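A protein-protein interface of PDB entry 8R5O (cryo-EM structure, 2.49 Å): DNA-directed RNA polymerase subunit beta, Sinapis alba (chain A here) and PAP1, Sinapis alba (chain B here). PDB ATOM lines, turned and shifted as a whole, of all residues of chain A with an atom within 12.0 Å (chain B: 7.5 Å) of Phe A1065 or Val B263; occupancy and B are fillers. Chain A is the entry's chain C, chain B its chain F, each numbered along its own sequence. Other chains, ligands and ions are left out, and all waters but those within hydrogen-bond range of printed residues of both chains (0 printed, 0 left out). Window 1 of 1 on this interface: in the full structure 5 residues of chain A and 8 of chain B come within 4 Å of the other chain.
The backbone carbonyl oxygen (O) of Glu A1062 sits close to a ring nitrogen (ND1) of His B226 (3.3 Å). O of Lys A1063 sits at hydrogen-bond distance from ND1 of His B226, 2.9 Å away. The backbone carbonyl oxygen (O) of Lys A1063 lies within hydrogen-bond range of the backbone NH (N) of Ser B227.
OG of Ser A1061 lies close to N of Lys A1063, 3.3 Å away. NE2 of His B226 is in hydrogen-bond range of NE2 of Gln B255 (3.0 Å). O of Val B254 is in hydrogen-bond range of OG1 of Thr B257 (2.9 Å). O of Val B263 lies close to OE1 of Gln B255. OE1 of Gln B255 sits at hydrogen-bond distance from OG1 of Thr B267 (2.7 Å). SG of Cys B258 sits close to N of Ile B260 (3.5 Å).
Among the printed residues, merely in contact across the chains: Phe A1065 with His B226 (3.3 Å), Glu A1062 with Leu B230 (3.5 Å), Phe A1065 with Cys B258 (3.6 Å), Phe A1065 with Gln B255 (3.6 Å), Phe A1065 with Val B263 (3.8 Å), Val A1060 with Ile B260 (3.8 Å), Phe A1065 with Val B254 (3.9 Å) and Ile A1067 with Ile B260 (3.9 Å).
Phe A1065 touches just these residues of chain B: His B226, Val B254, Gln B255, Cys B258 and Val B263. Of chain A, only Phe A1065 comes within 4 Å of Val B254. No residue of chain A comes within 4 Å of Gly B259. Ile B260 touches two residues of chain A. No residue of chain A comes within 4 Å of Pro B261. No residue of chain A comes within 4 Å of Ala B264. No residue of chain A comes within 4 Å of Ala B266. Printed residues of chain A within 4 Å of Leu B230: Glu A1062. Of the printed residues of chain B, Lys A1063 touches His B226 (2.9 Å) and Ser B227 (3.4 Å). Printed residues of chain B within 4 Å of Val A1060: Ile B260 (3.8 Å). Gln A1066 touches none of the printed residues of chain B. Asn A1068 touches none of the printed residues of chain B. The nearest printed residue of chain B that does not touch Val A1060 is Val B263 (4.1 Å).
Printed residues of chain B that touch a printed residue of chain A: His B226, Ser B227, Leu B230, Val B254, Gln B255, Cys B258, Ile B260 and Val B263. Hydrophobic or aromatic side chains of chain A that line the printed part of chain B: Val A1060, Phe A1065 and Ile A1067. Among the printed residues, no Asp or Glu carboxylate lies within 4 Å of a Lys or Arg side-chain nitrogen of the other chain.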
ATOM      1  N   PHE A1058     -22.649 -20.474 -20.787  1.00  0.00           N
ATOM      2  CA  PHE A1058     -22.584 -19.775 -19.512  1.00  0.00           C
ATOM      3  C   PHE A1058     -22.699 -20.763 -18.361  1.00  0.00           C
ATOM      4  O   PHE A1058     -23.524 -21.681 -18.396  1.00  0.00           O
ATOM      5  CB  PHE A1058     -23.693 -18.728 -19.393  1.00  0.00           C
ATOM      6  CG  PHE A1058     -23.563 -17.589 -20.357  1.00  0.00           C
ATOM      7  CD1 PHE A1058     -22.588 -16.624 -20.182  1.00  0.00           C
ATOM      8  CD2 PHE A1058     -24.426 -17.475 -21.433  1.00  0.00           C
ATOM      9  CE1 PHE A1058     -22.470 -15.571 -21.066  1.00  0.00           C
ATOM     10  CE2 PHE A1058     -24.314 -16.425 -22.318  1.00  0.00           C
ATOM     11  CZ  PHE A1058     -23.335 -15.472 -22.134  1.00  0.00           C
ATOM     12  N   LEU A1059     -21.866 -20.568 -17.344  1.00  0.00           N
ATOM     13  CA  LEU A1059     -21.951 -21.314 -16.097  1.00  0.00           C
ATOM     14  C   LEU A1059     -22.481 -20.395 -15.008  1.00  0.00           C
ATOM     15  O   LEU A1059     -21.926 -19.316 -14.779  1.00  0.00           O
ATOM     16  CB  LEU A1059     -20.590 -21.877 -15.688  1.00  0.00           C
ATOM     17  CG  LEU A1059     -19.894 -22.825 -16.664  1.00  0.00           C
ATOM     18  CD1 LEU A1059     -18.620 -23.386 -16.050  1.00  0.00           C
ATOM     19  CD2 LEU A1059     -20.828 -23.944 -17.079  1.00  0.00           C
ATOM     20  N   VAL A1060     -23.548 -20.820 -14.345  1.00  0.00           N
ATOM     21  CA  VAL A1060     -24.119 -20.082 -13.226  1.00  0.00           C
ATOM     22  C   VAL A1060     -23.662 -20.759 -11.944  1.00  0.00           C
ATOM     23  O   VAL A1060     -23.945 -21.942 -11.723  1.00  0.00           O
ATOM     24  CB  VAL A1060     -25.651 -20.025 -13.309  1.00  0.00           C
ATOM     25  CG1 VAL A1060     -26.210 -19.237 -12.139  1.00  0.00           C
ATOM     26  CG2 VAL A1060     -26.084 -19.418 -14.631  1.00  0.00           C
ATOM     27  N   SER A1061     -22.951 -20.013 -11.105  1.00  0.00           N
ATOM     28  CA  SER A1061     -22.453 -20.568  -9.856  1.00  0.00           C
ATOM     29  C   SER A1061     -23.609 -20.831  -8.901  1.00  0.00           C
ATOM     30  O   SER A1061     -24.466 -19.969  -8.694  1.00  0.00           O
ATOM     31  CB  SER A1061     -21.444 -19.615  -9.218  1.00  0.00           C
ATOM     32  OG  SER A1061     -20.980 -20.120  -7.980  1.00  0.00           O
ATOM     33  N   GLU A1062     -23.634 -22.030  -8.321  1.00  0.00           N
ATOM     34  CA  GLU A1062     -24.664 -22.352  -7.344  1.00  0.00           C
ATOM     35  C   GLU A1062     -24.423 -21.680  -6.000  1.00  0.00           C
ATOM     36  O   GLU A1062     -25.327 -21.679  -5.158  1.00  0.00           O
ATOM     37  CB  GLU A1062     -24.768 -23.869  -7.154  1.00  0.00           C
ATOM     38  CG  GLU A1062     -23.535 -24.523  -6.551  1.00  0.00           C
ATOM     39  CD  GLU A1062     -22.414 -24.704  -7.554  1.00  0.00           C
ATOM     40  OE1 GLU A1062     -22.693 -24.676  -8.771  1.00  0.00           O
ATOM     41  OE2 GLU A1062     -21.253 -24.872  -7.126  1.00  0.00           O
ATOM     42  N   LYS A1063     -23.240 -21.106  -5.784  1.00  0.00           N
ATOM     43  CA  LYS A1063     -22.914 -20.459  -4.517  1.00  0.00           C
ATOM     44  C   LYS A1063     -23.323 -18.987  -4.503  1.00  0.00           C
ATOM     45  O   LYS A1063     -24.130 -18.571  -3.667  1.00  0.00           O
ATOM     46  CB  LYS A1063     -21.416 -20.603  -4.228  1.00  0.00           C
ATOM     47  CG  LYS A1063     -20.912 -22.032  -4.278  1.00  0.00           C
ATOM     48  CD  LYS A1063     -19.431 -22.103  -3.944  1.00  0.00           C
ATOM     49  CE  LYS A1063     -18.887 -23.507  -4.142  1.00  0.00           C
ATOM     50  NZ  LYS A1063     -18.996 -23.945  -5.559  1.00  0.00           N
ATOM     51  N   ASN A1064     -22.781 -18.191  -5.425  1.00  0.00           N
ATOM     52  CA  ASN A1064     -23.019 -16.753  -5.442  1.00  0.00           C
ATOM     53  C   ASN A1064     -23.799 -16.276  -6.660  1.00  0.00           C
ATOM     54  O   ASN A1064     -23.957 -15.063  -6.836  1.00  0.00           O
ATOM     55  CB  ASN A1064     -21.689 -15.993  -5.348  1.00  0.00           C
ATOM     56  CG  ASN A1064     -20.678 -16.444  -6.385  1.00  0.00           C
ATOM     57  OD1 ASN A1064     -21.030 -16.760  -7.521  1.00  0.00           O
ATOM     58  ND2 ASN A1064     -19.411 -16.480  -5.994  1.00  0.00           N
ATOM     59  N   PHE A1065     -24.272 -17.189  -7.511  1.00  0.00           N
ATOM     60  CA  PHE A1065     -25.159 -16.891  -8.633  1.00  0.00           C
ATOM     61  C   PHE A1065     -24.503 -16.025  -9.702  1.00  0.00           C
ATOM     62  O   PHE A1065     -25.203 -15.374 -10.484  1.00  0.00           O
ATOM     63  CB  PHE A1065     -26.456 -16.228  -8.157  1.00  0.00           C
ATOM     64  CG  PHE A1065     -27.044 -16.857  -6.929  1.00  0.00           C
ATOM     65  CD1 PHE A1065     -27.186 -18.230  -6.837  1.00  0.00           C
ATOM     66  CD2 PHE A1065     -27.440 -16.073  -5.859  1.00  0.00           C
ATOM     67  CE1 PHE A1065     -27.721 -18.807  -5.707  1.00  0.00           C
ATOM     68  CE2 PHE A1065     -27.976 -16.646  -4.726  1.00  0.00           C
ATOM     69  CZ  PHE A1065     -28.117 -18.015  -4.651  1.00  0.00           C
ATOM     70  N   GLN A1066     -23.177 -16.000  -9.764  1.00  0.00           N
ATOM     71  CA  GLN A1066     -22.474 -15.198 -10.753  1.00  0.00           C
ATOM     72  C   GLN A1066     -22.294 -15.989 -12.041  1.00  0.00           C
ATOM     73  O   GLN A1066     -21.944 -17.173 -12.017  1.00  0.00           O
ATOM     74  CB  GLN A1066     -21.118 -14.743 -10.214  1.00  0.00           C
ATOM     75  CG  GLN A1066     -21.227 -13.786  -9.041  1.00  0.00           C
ATOM     76  CD  GLN A1066     -19.876 -13.401  -8.473  1.00  0.00           C
ATOM     77  OE1 GLN A1066     -18.835 -13.792  -8.998  1.00  0.00           O
ATOM     78  NE2 GLN A1066     -19.888 -12.629  -7.392  1.00  0.00           N
ATOM     79  N   ILE A1067     -22.533 -15.325 -13.163  1.00  0.00           N
ATOM     80  CA  ILE A1067     -22.516 -15.968 -14.471  1.00  0.00           C
ATOM     81  C   ILE A1067     -21.126 -15.836 -15.075  1.00  0.00           C
ATOM     82  O   ILE A1067     -20.562 -14.738 -15.131  1.00  0.00           O
ATOM     83  CB  ILE A1067     -23.580 -15.352 -15.394  1.00  0.00           C
ATOM     84  CG1 ILE A1067     -24.958 -15.444 -14.740  1.00  0.00           C
ATOM     85  CG2 ILE A1067     -23.576 -16.046 -16.744  1.00  0.00           C
ATOM     86  CD1 ILE A1067     -26.062 -14.837 -15.560  1.00  0.00           C
ATOM     87  N   ASN A1068     -20.573 -16.958 -15.525  1.00  0.00           N
ATOM     88  CA  ASN A1068     -19.256 -16.999 -16.144  1.00  0.00           C
ATOM     89  C   ASN A1068     -19.395 -17.463 -17.585  1.00  0.00           C
ATOM     90  O   ASN A1068     -19.987 -18.514 -17.848  1.00  0.00           O
ATOM     91  CB  ASN A1068     -18.316 -17.930 -15.376  1.00  0.00           C
ATOM     92  CG  ASN A1068     -18.113 -17.497 -13.938  1.00  0.00           C
ATOM     93  OD1 ASN A1068     -18.113 -16.305 -13.631  1.00  0.00           O
ATOM     94  ND2 ASN A1068     -17.939 -18.466 -13.046  1.00  0.00           N
ATOM     95  N   ARG A1069     -18.853 -16.680 -18.514  1.00  0.00           N
ATOM     96  CA  ARG A1069     -18.854 -17.032 -19.929  1.00  0.00           C
ATOM     97  C   ARG A1069     -17.620 -17.879 -20.215  1.00  0.00           C
ATOM     98  O   ARG A1069     -16.489 -17.392 -20.114  1.00  0.00           O
ATOM     99  CB  ARG A1069     -18.875 -15.778 -20.799  1.00  0.00           C
ATOM    100  CG  ARG A1069     -18.826 -16.056 -22.291  1.00  0.00           C
ATOM    101  CD  ARG A1069     -18.557 -14.787 -23.083  1.00  0.00           C
ATOM    102  NE  ARG A1069     -19.703 -13.885 -23.095  1.00  0.00           N
ATOM    103  CZ  ARG A1069     -20.523 -13.735 -24.126  1.00  0.00           C
ATOM    104  NH1 ARG A1069     -20.348 -14.405 -25.252  1.00  0.00           N
ATOM    105  NH2 ARG A1069     -21.542 -12.885 -24.026  1.00  0.00           N
ATOM    106  N   GLY B 224     -27.576 -12.311   3.135  1.00  0.00           N
ATOM    107  CA  GLY B 224     -27.351 -12.483   1.715  1.00  0.00           C
ATOM    108  C   GLY B 224     -26.136 -13.307   1.360  1.00  0.00           C
ATOM    109  O   GLY B 224     -25.653 -13.223   0.230  1.00  0.00           O
ATOM    110  N   ASP B 225     -25.625 -14.105   2.297  1.00  0.00           N
ATOM    111  CA  ASP B 225     -24.435 -14.921   2.062  1.00  0.00           C
ATOM    112  C   ASP B 225     -24.884 -16.347   1.758  1.00  0.00           C
ATOM    113  O   ASP B 225     -24.895 -17.228   2.618  1.00  0.00           O
ATOM    114  CB  ASP B 225     -23.499 -14.860   3.264  1.00  0.00           C
ATOM    115  CG  ASP B 225     -22.146 -15.475   2.983  1.00  0.00           C
ATOM    116  OD1 ASP B 225     -21.915 -15.923   1.840  1.00  0.00           O
ATOM    117  OD2 ASP B 225     -21.309 -15.509   3.907  1.00  0.00           O
ATOM    118  N   HIS B 226     -25.257 -16.570   0.498  1.00  0.00           N
ATOM    119  CA  HIS B 226     -25.695 -17.897   0.082  1.00  0.00           C
ATOM    120  C   HIS B 226     -24.527 -18.867  -0.032  1.00  0.00           C
ATOM    121  O   HIS B 226     -24.704 -20.073   0.172  1.00  0.00           O
ATOM    122  CB  HIS B 226     -26.444 -17.807  -1.247  1.00  0.00           C
ATOM    123  CG  HIS B 226     -27.054 -19.101  -1.687  1.00  0.00           C
ATOM    124  ND1 HIS B 226     -26.386 -20.009  -2.479  1.00  0.00           N
ATOM    125  CD2 HIS B 226     -28.275 -19.636  -1.450  1.00  0.00           C
ATOM    126  CE1 HIS B 226     -27.166 -21.048  -2.708  1.00  0.00           C
ATOM    127  NE2 HIS B 226     -28.318 -20.847  -2.095  1.00  0.00           N
ATOM    128  N   SER B 227     -23.335 -18.365  -0.362  1.00  0.00           N
ATOM    129  CA  SER B 227     -22.186 -19.243  -0.550  1.00  0.00           C
ATOM    130  C   SER B 227     -21.800 -19.945   0.747  1.00  0.00           C
ATOM    131  O   SER B 227     -21.492 -21.141   0.744  1.00  0.00           O
ATOM    132  CB  SER B 227     -21.006 -18.445  -1.101  1.00  0.00           C
ATOM    133  OG  SER B 227     -19.871 -19.273  -1.279  1.00  0.00           O
ATOM    134  N   LEU B 230     -24.741 -22.382   1.858  1.00  0.00           N
ATOM    135  CA  LEU B 230     -24.771 -23.632   1.108  1.00  0.00           C
ATOM    136  C   LEU B 230     -23.622 -24.550   1.511  1.00  0.00           C
ATOM    137  O   LEU B 230     -23.788 -25.774   1.545  1.00  0.00           O
ATOM    138  CB  LEU B 230     -24.733 -23.346  -0.393  1.00  0.00           C
ATOM    139  CG  LEU B 230     -24.975 -24.542  -1.315  1.00  0.00           C
ATOM    140  CD1 LEU B 230     -26.354 -25.135  -1.078  1.00  0.00           C
ATOM    141  CD2 LEU B 230     -24.806 -24.139  -2.770  1.00  0.00           C
ATOM    142  N   LEU B 251     -32.213 -20.892   2.158  1.00  0.00           N
ATOM    143  CA  LEU B 251     -31.503 -20.759   0.889  1.00  0.00           C
ATOM    144  C   LEU B 251     -32.386 -20.120  -0.175  1.00  0.00           C
ATOM    145  O   LEU B 251     -31.913 -19.300  -0.969  1.00  0.00           O
ATOM    146  CB  LEU B 251     -31.001 -22.125   0.422  1.00  0.00           C
ATOM    147  CG  LEU B 251     -30.045 -22.866   1.356  1.00  0.00           C
ATOM    148  CD1 LEU B 251     -29.701 -24.234   0.792  1.00  0.00           C
ATOM    149  CD2 LEU B 251     -28.785 -22.052   1.592  1.00  0.00           C
ATOM    150  N   LEU B 252     -33.671 -20.484  -0.210  1.00  0.00           N
ATOM    151  CA  LEU B 252     -34.577 -19.921  -1.205  1.00  0.00           C
ATOM    152  C   LEU B 252     -34.778 -18.426  -1.006  1.00  0.00           C
ATOM    153  O   LEU B 252     -35.052 -17.708  -1.974  1.00  0.00           O
ATOM    154  CB  LEU B 252     -35.923 -20.640  -1.162  1.00  0.00           C
ATOM    155  CG  LEU B 252     -35.982 -21.997  -1.859  1.00  0.00           C
ATOM    156  CD1 LEU B 252     -37.339 -22.642  -1.655  1.00  0.00           C
ATOM    157  CD2 LEU B 252     -35.676 -21.841  -3.339  1.00  0.00           C
ATOM    158  N   SER B 253     -34.651 -17.941   0.230  1.00  0.00           N
ATOM    159  CA  SER B 253     -34.814 -16.516   0.488  1.00  0.00           C
ATOM    160  C   SER B 253     -33.778 -15.689  -0.264  1.00  0.00           C
ATOM    161  O   SER B 253     -34.031 -14.523  -0.585  1.00  0.00           O
ATOM    162  CB  SER B 253     -34.733 -16.242   1.988  1.00  0.00           C
ATOM    163  OG  SER B 253     -33.486 -16.647   2.521  1.00  0.00           O
ATOM    164  N   VAL B 254     -32.620 -16.270  -0.558  1.00  0.00           N
ATOM    165  CA  VAL B 254     -31.575 -15.588  -1.306  1.00  0.00           C
ATOM    166  C   VAL B 254     -31.619 -15.944  -2.787  1.00  0.00           C
ATOM    167  O   VAL B 254     -31.340 -15.101  -3.637  1.00  0.00           O
ATOM    168  CB  VAL B 254     -30.193 -15.907  -0.695  1.00  0.00           C
ATOM    169  CG1 VAL B 254     -29.116 -15.045  -1.328  1.00  0.00           C
ATOM    170  CG2 VAL B 254     -30.225 -15.711   0.811  1.00  0.00           C
ATOM    171  N   GLN B 255     -31.973 -17.191  -3.109  1.00  0.00           N
ATOM    172  CA  GLN B 255     -32.032 -17.613  -4.504  1.00  0.00           C
ATOM    173  C   GLN B 255     -33.125 -16.885  -5.277  1.00  0.00           C
ATOM    174  O   GLN B 255     -33.002 -16.700  -6.491  1.00  0.00           O
ATOM    175  CB  GLN B 255     -32.251 -19.122  -4.590  1.00  0.00           C
ATOM    176  CG  GLN B 255     -31.130 -19.959  -4.008  1.00  0.00           C
ATOM    177  CD  GLN B 255     -31.438 -21.440  -4.054  1.00  0.00           C
ATOM    178  OE1 GLN B 255     -32.409 -21.860  -4.678  1.00  0.00           O
ATOM    179  NE2 GLN B 255     -30.616 -22.238  -3.389  1.00  0.00           N
ATOM    180  N   ALA B 256     -34.197 -16.473  -4.600  1.00  0.00           N
ATOM    181  CA  ALA B 256     -35.311 -15.822  -5.277  1.00  0.00           C
ATOM    182  C   ALA B 256     -34.988 -14.405  -5.732  1.00  0.00           C
ATOM    183  O   ALA B 256     -35.767 -13.830  -6.499  1.00  0.00           O
ATOM    184  CB  ALA B 256     -36.538 -15.802  -4.364  1.00  0.00           C
ATOM    185  N   THR B 257     -33.871 -13.832  -5.290  1.00  0.00           N
ATOM    186  CA  THR B 257     -33.506 -12.464  -5.630  1.00  0.00           C
ATOM    187  C   THR B 257     -32.345 -12.384  -6.615  1.00  0.00           C
ATOM    188  O   THR B 257     -31.849 -11.285  -6.880  1.00  0.00           O
ATOM    189  CB  THR B 257     -33.165 -11.678  -4.362  1.00  0.00           C
ATOM    190  OG1 THR B 257     -32.014 -12.255  -3.736  1.00  0.00           O
ATOM    191  CG2 THR B 257     -34.330 -11.713  -3.389  1.00  0.00           C
ATOM    192  N   CYS B 258     -31.900 -13.512  -7.165  1.00  0.00           N
ATOM    193  CA  CYS B 258     -30.757 -13.514  -8.068  1.00  0.00           C
ATOM    194  C   CYS B 258     -31.130 -13.232  -9.519  1.00  0.00           C
ATOM    195  O   CYS B 258     -30.232 -13.073 -10.351  1.00  0.00           O
ATOM    196  CB  CYS B 258     -30.015 -14.852  -7.989  1.00  0.00           C
ATOM    197  SG  CYS B 258     -30.856 -16.241  -8.784  1.00  0.00           S
ATOM    198  N   GLY B 259     -32.419 -13.168  -9.843  1.00  0.00           N
ATOM    199  CA  GLY B 259     -32.845 -12.880 -11.195  1.00  0.00           C
ATOM    200  C   GLY B 259     -32.845 -14.060 -12.143  1.00  0.00           C
ATOM    201  O   GLY B 259     -33.215 -13.890 -13.310  1.00  0.00           O
ATOM    202  N   ILE B 260     -32.445 -15.239 -11.688  1.00  0.00           N
ATOM    203  CA  ILE B 260     -32.460 -16.452 -12.491  1.00  0.00           C
ATOM    204  C   ILE B 260     -33.426 -17.435 -11.843  1.00  0.00           C
ATOM    205  O   ILE B 260     -33.094 -18.087 -10.852  1.00  0.00           O
ATOM    206  CB  ILE B 260     -31.053 -17.061 -12.623  1.00  0.00           C
ATOM    207  CG1 ILE B 260     -30.053 -15.993 -13.064  1.00  0.00           C
ATOM    208  CG2 ILE B 260     -31.062 -18.220 -13.608  1.00  0.00           C
ATOM    209  CD1 ILE B 260     -28.643 -16.502 -13.200  1.00  0.00           C
ATOM    210  N   PRO B 261     -34.644 -17.562 -12.373  1.00  0.00           N
ATOM    211  CA  PRO B 261     -35.643 -18.422 -11.717  1.00  0.00           C
ATOM    212  C   PRO B 261     -35.269 -19.892 -11.691  1.00  0.00           C
ATOM    213  O   PRO B 261     -35.783 -20.627 -10.842  1.00  0.00           O
ATOM    214  CB  PRO B 261     -36.912 -18.190 -12.551  1.00  0.00           C
ATOM    215  CG  PRO B 261     -36.638 -16.983 -13.378  1.00  0.00           C
ATOM    216  CD  PRO B 261     -35.168 -16.949 -13.601  1.00  0.00           C
ATOM    217  N   GLU B 262     -34.395 -20.345 -12.592  1.00  0.00           N
ATOM    218  CA  GLU B 262     -34.050 -21.761 -12.636  1.00  0.00           C
ATOM    219  C   GLU B 262     -33.238 -22.183 -11.420  1.00  0.00           C
ATOM    220  O   GLU B 262     -33.267 -23.358 -11.037  1.00  0.00           O
ATOM    221  CB  GLU B 262     -33.290 -22.079 -13.923  1.00  0.00           C
ATOM    222  CG  GLU B 262     -34.149 -22.060 -15.180  1.00  0.00           C
ATOM    223  CD  GLU B 262     -34.493 -20.657 -15.652  1.00  0.00           C
ATOM    224  OE1 GLU B 262     -33.843 -19.691 -15.202  1.00  0.00           O
ATOM    225  OE2 GLU B 262     -35.418 -20.521 -16.478  1.00  0.00           O
ATOM    226  N   VAL B 263     -32.501 -21.254 -10.811  1.00  0.00           N
ATOM    227  CA  VAL B 263     -31.749 -21.573  -9.602  1.00  0.00           C
ATOM    228  C   VAL B 263     -32.697 -21.921  -8.463  1.00  0.00           C
ATOM    229  O   VAL B 263     -32.523 -22.929  -7.772  1.00  0.00           O
ATOM    230  CB  VAL B 263     -30.819 -20.407  -9.227  1.00  0.00           C
ATOM    231  CG1 VAL B 263     -30.152 -20.668  -7.888  1.00  0.00           C
ATOM    232  CG2 VAL B 263     -29.779 -20.187 -10.313  1.00  0.00           C
ATOM    233  N   ALA B 264     -33.720 -21.090  -8.254  1.00  0.00           N
ATOM    234  CA  ALA B 264     -34.679 -21.351  -7.189  1.00  0.00           C
ATOM    235  C   ALA B 264     -35.553 -22.557  -7.499  1.00  0.00           C
ATOM    236  O   ALA B 264     -35.967 -23.272  -6.582  1.00  0.00           O
ATOM    237  CB  ALA B 264     -35.545 -20.117  -6.949  1.00  0.00           C
ATOM    238  N   TYR B 265     -35.848 -22.798  -8.778  1.00  0.00           N
ATOM    239  CA  TYR B 265     -36.714 -23.916  -9.132  1.00  0.00           C
ATOM    240  C   TYR B 265     -36.011 -25.255  -8.954  1.00  0.00           C
ATOM    241  O   TYR B 265     -36.669 -26.265  -8.685  1.00  0.00           O
ATOM    242  CB  TYR B 265     -37.214 -23.761 -10.565  1.00  0.00           C
ATOM    243  CG  TYR B 265     -38.265 -24.769 -10.946  1.00  0.00           C
ATOM    244  CD1 TYR B 265     -39.550 -24.684 -10.433  1.00  0.00           C
ATOM    245  CD2 TYR B 265     -37.977 -25.808 -11.816  1.00  0.00           C
ATOM    246  CE1 TYR B 265     -40.516 -25.604 -10.775  1.00  0.00           C
ATOM    247  CE2 TYR B 265     -38.936 -26.731 -12.165  1.00  0.00           C
ATOM    248  CZ  TYR B 265     -40.205 -26.626 -11.640  1.00  0.00           C
ATOM    249  OH  TYR B 265     -41.166 -27.544 -11.986  1.00  0.00           O
ATOM    250  N   ALA B 266     -34.687 -25.288  -9.110  1.00  0.00           N
ATOM    251  CA  ALA B 266     -33.942 -26.514  -8.846  1.00  0.00           C
ATOM    252  C   ALA B 266     -34.023 -26.900  -7.374  1.00  0.00           C
ATOM    253  O   ALA B 266     -34.168 -28.082  -7.045  1.00  0.00           O
ATOM    254  CB  ALA B 266     -32.488 -26.352  -9.283  1.00  0.00           C
ATOM    255  N   THR B 267     -33.923 -25.917  -6.476  1.00  0.00           N
ATOM    256  CA  THR B 267     -34.087 -26.190  -5.051  1.00  0.00           C
ATOM    257  C   THR B 267     -35.505 -26.652  -4.739  1.00  0.00           C
ATOM    258  O   THR B 267     -35.706 -27.558  -3.923  1.00  0.00           O
ATOM    259  CB  THR B 267     -33.734 -24.946  -4.235  1.00  0.00           C
ATOM    260  OG1 THR B 267     -32.380 -24.569  -4.504  1.00  0.00           O
ATOM    261  CG2 THR B 267     -33.894 -25.208  -2.746  1.00  0.00           C
ATOM    262  N   PHE B 268     -36.502 -26.038  -5.378  1.00  0.00           N
ATOM    263  CA  PHE B 268     -37.887 -26.437  -5.154  1.00  0.00           C
ATOM    264  C   PHE B 268     -38.122 -27.886  -5.565  1.00  0.00           C
ATOM    265  O   PHE B 268     -38.826 -28.627  -4.872  1.00  0.00           O
ATOM    266  CB  PHE B 268     -38.831 -25.501  -5.911  1.00  0.00           C
ATOM    267  CG  PHE B 268     -40.269 -25.935  -5.882  1.00  0.00           C
ATOM    268  CD1 PHE B 268     -41.056 -25.691  -4.772  1.00  0.00           C
ATOM    269  CD2 PHE B 268     -40.833 -26.584  -6.968  1.00  0.00           C
ATOM    270  CE1 PHE B 268     -42.376 -26.090  -4.742  1.00  0.00           C
ATOM    271  CE2 PHE B 268     -42.150 -26.984  -6.943  1.00  0.00           C
ATOM    272  CZ  PHE B 268     -42.923 -26.737  -5.828  1.00  0.00           C
ATOM    273  N   GLU B 269     -37.546 -28.306  -6.694  1.00  0.00           N
ATOM    274  CA  GLU B 269     -37.698 -29.691  -7.127  1.00  0.00           C
ATOM    275  C   GLU B 269     -37.018 -30.656  -6.167  1.00  0.00           C
ATOM    276  O   GLU B 269     -37.495 -31.780  -5.980  1.00  0.00           O
ATOM    277  CB  GLU B 269     -37.147 -29.869  -8.541  1.00  0.00           C
ATOM    278  CG  GLU B 269     -38.019 -29.263  -9.624  1.00  0.00           C
ATOM    279  CD  GLU B 269     -37.481 -29.515 -11.018  1.00  0.00           C
ATOM    280  OE1 GLU B 269     -36.251 -29.411 -11.211  1.00  0.00           O
ATOM    281  OE2 GLU B 269     -38.287 -29.820 -11.922  1.00  0.00           O
ATOM    282  N   ALA B 291     -39.553 -15.709  -7.508  1.00  0.00           N
ATOM    283  CA  ALA B 291     -38.415 -15.781  -8.417  1.00  0.00           C
ATOM    284  C   ALA B 291     -38.853 -15.626  -9.868  1.00  0.00           C
ATOM    285  O   ALA B 291     -38.189 -14.942 -10.654  1.00  0.00           O
ATOM    286  CB  ALA B 291     -37.669 -17.098  -8.217  1.00  0.00           C
ATOM    287  N   TYR B 292     -39.971 -16.250 -10.242  1.00  0.00           N
ATOM    288  CA  TYR B 292     -40.443 -16.163 -11.619  1.00  0.00           C
ATOM    289  C   TYR B 292     -41.101 -14.820 -11.916  1.00  0.00           C
ATOM    290  O   TYR B 292     -40.964 -14.296 -13.026  1.00  0.00           O
ATOM    291  CB  TYR B 292     -41.410 -17.309 -11.918  1.00  0.00           C
ATOM    292  CG  TYR B 292     -40.721 -18.604 -12.274  1.00  0.00           C
ATOM    293  CD1 TYR B 292     -40.226 -18.817 -13.552  1.00  0.00           C
ATOM    294  CD2 TYR B 292     -40.564 -19.613 -11.337  1.00  0.00           C
ATOM    295  CE1 TYR B 292     -39.592 -19.995 -13.886  1.00  0.00           C
ATOM    296  CE2 TYR B 292     -39.932 -20.798 -11.663  1.00  0.00           C
ATOM    297  CZ  TYR B 292     -39.448 -20.982 -12.939  1.00  0.00           C
ATOM    298  OH  TYR B 292     -38.817 -22.158 -13.270  1.00  0.00           O
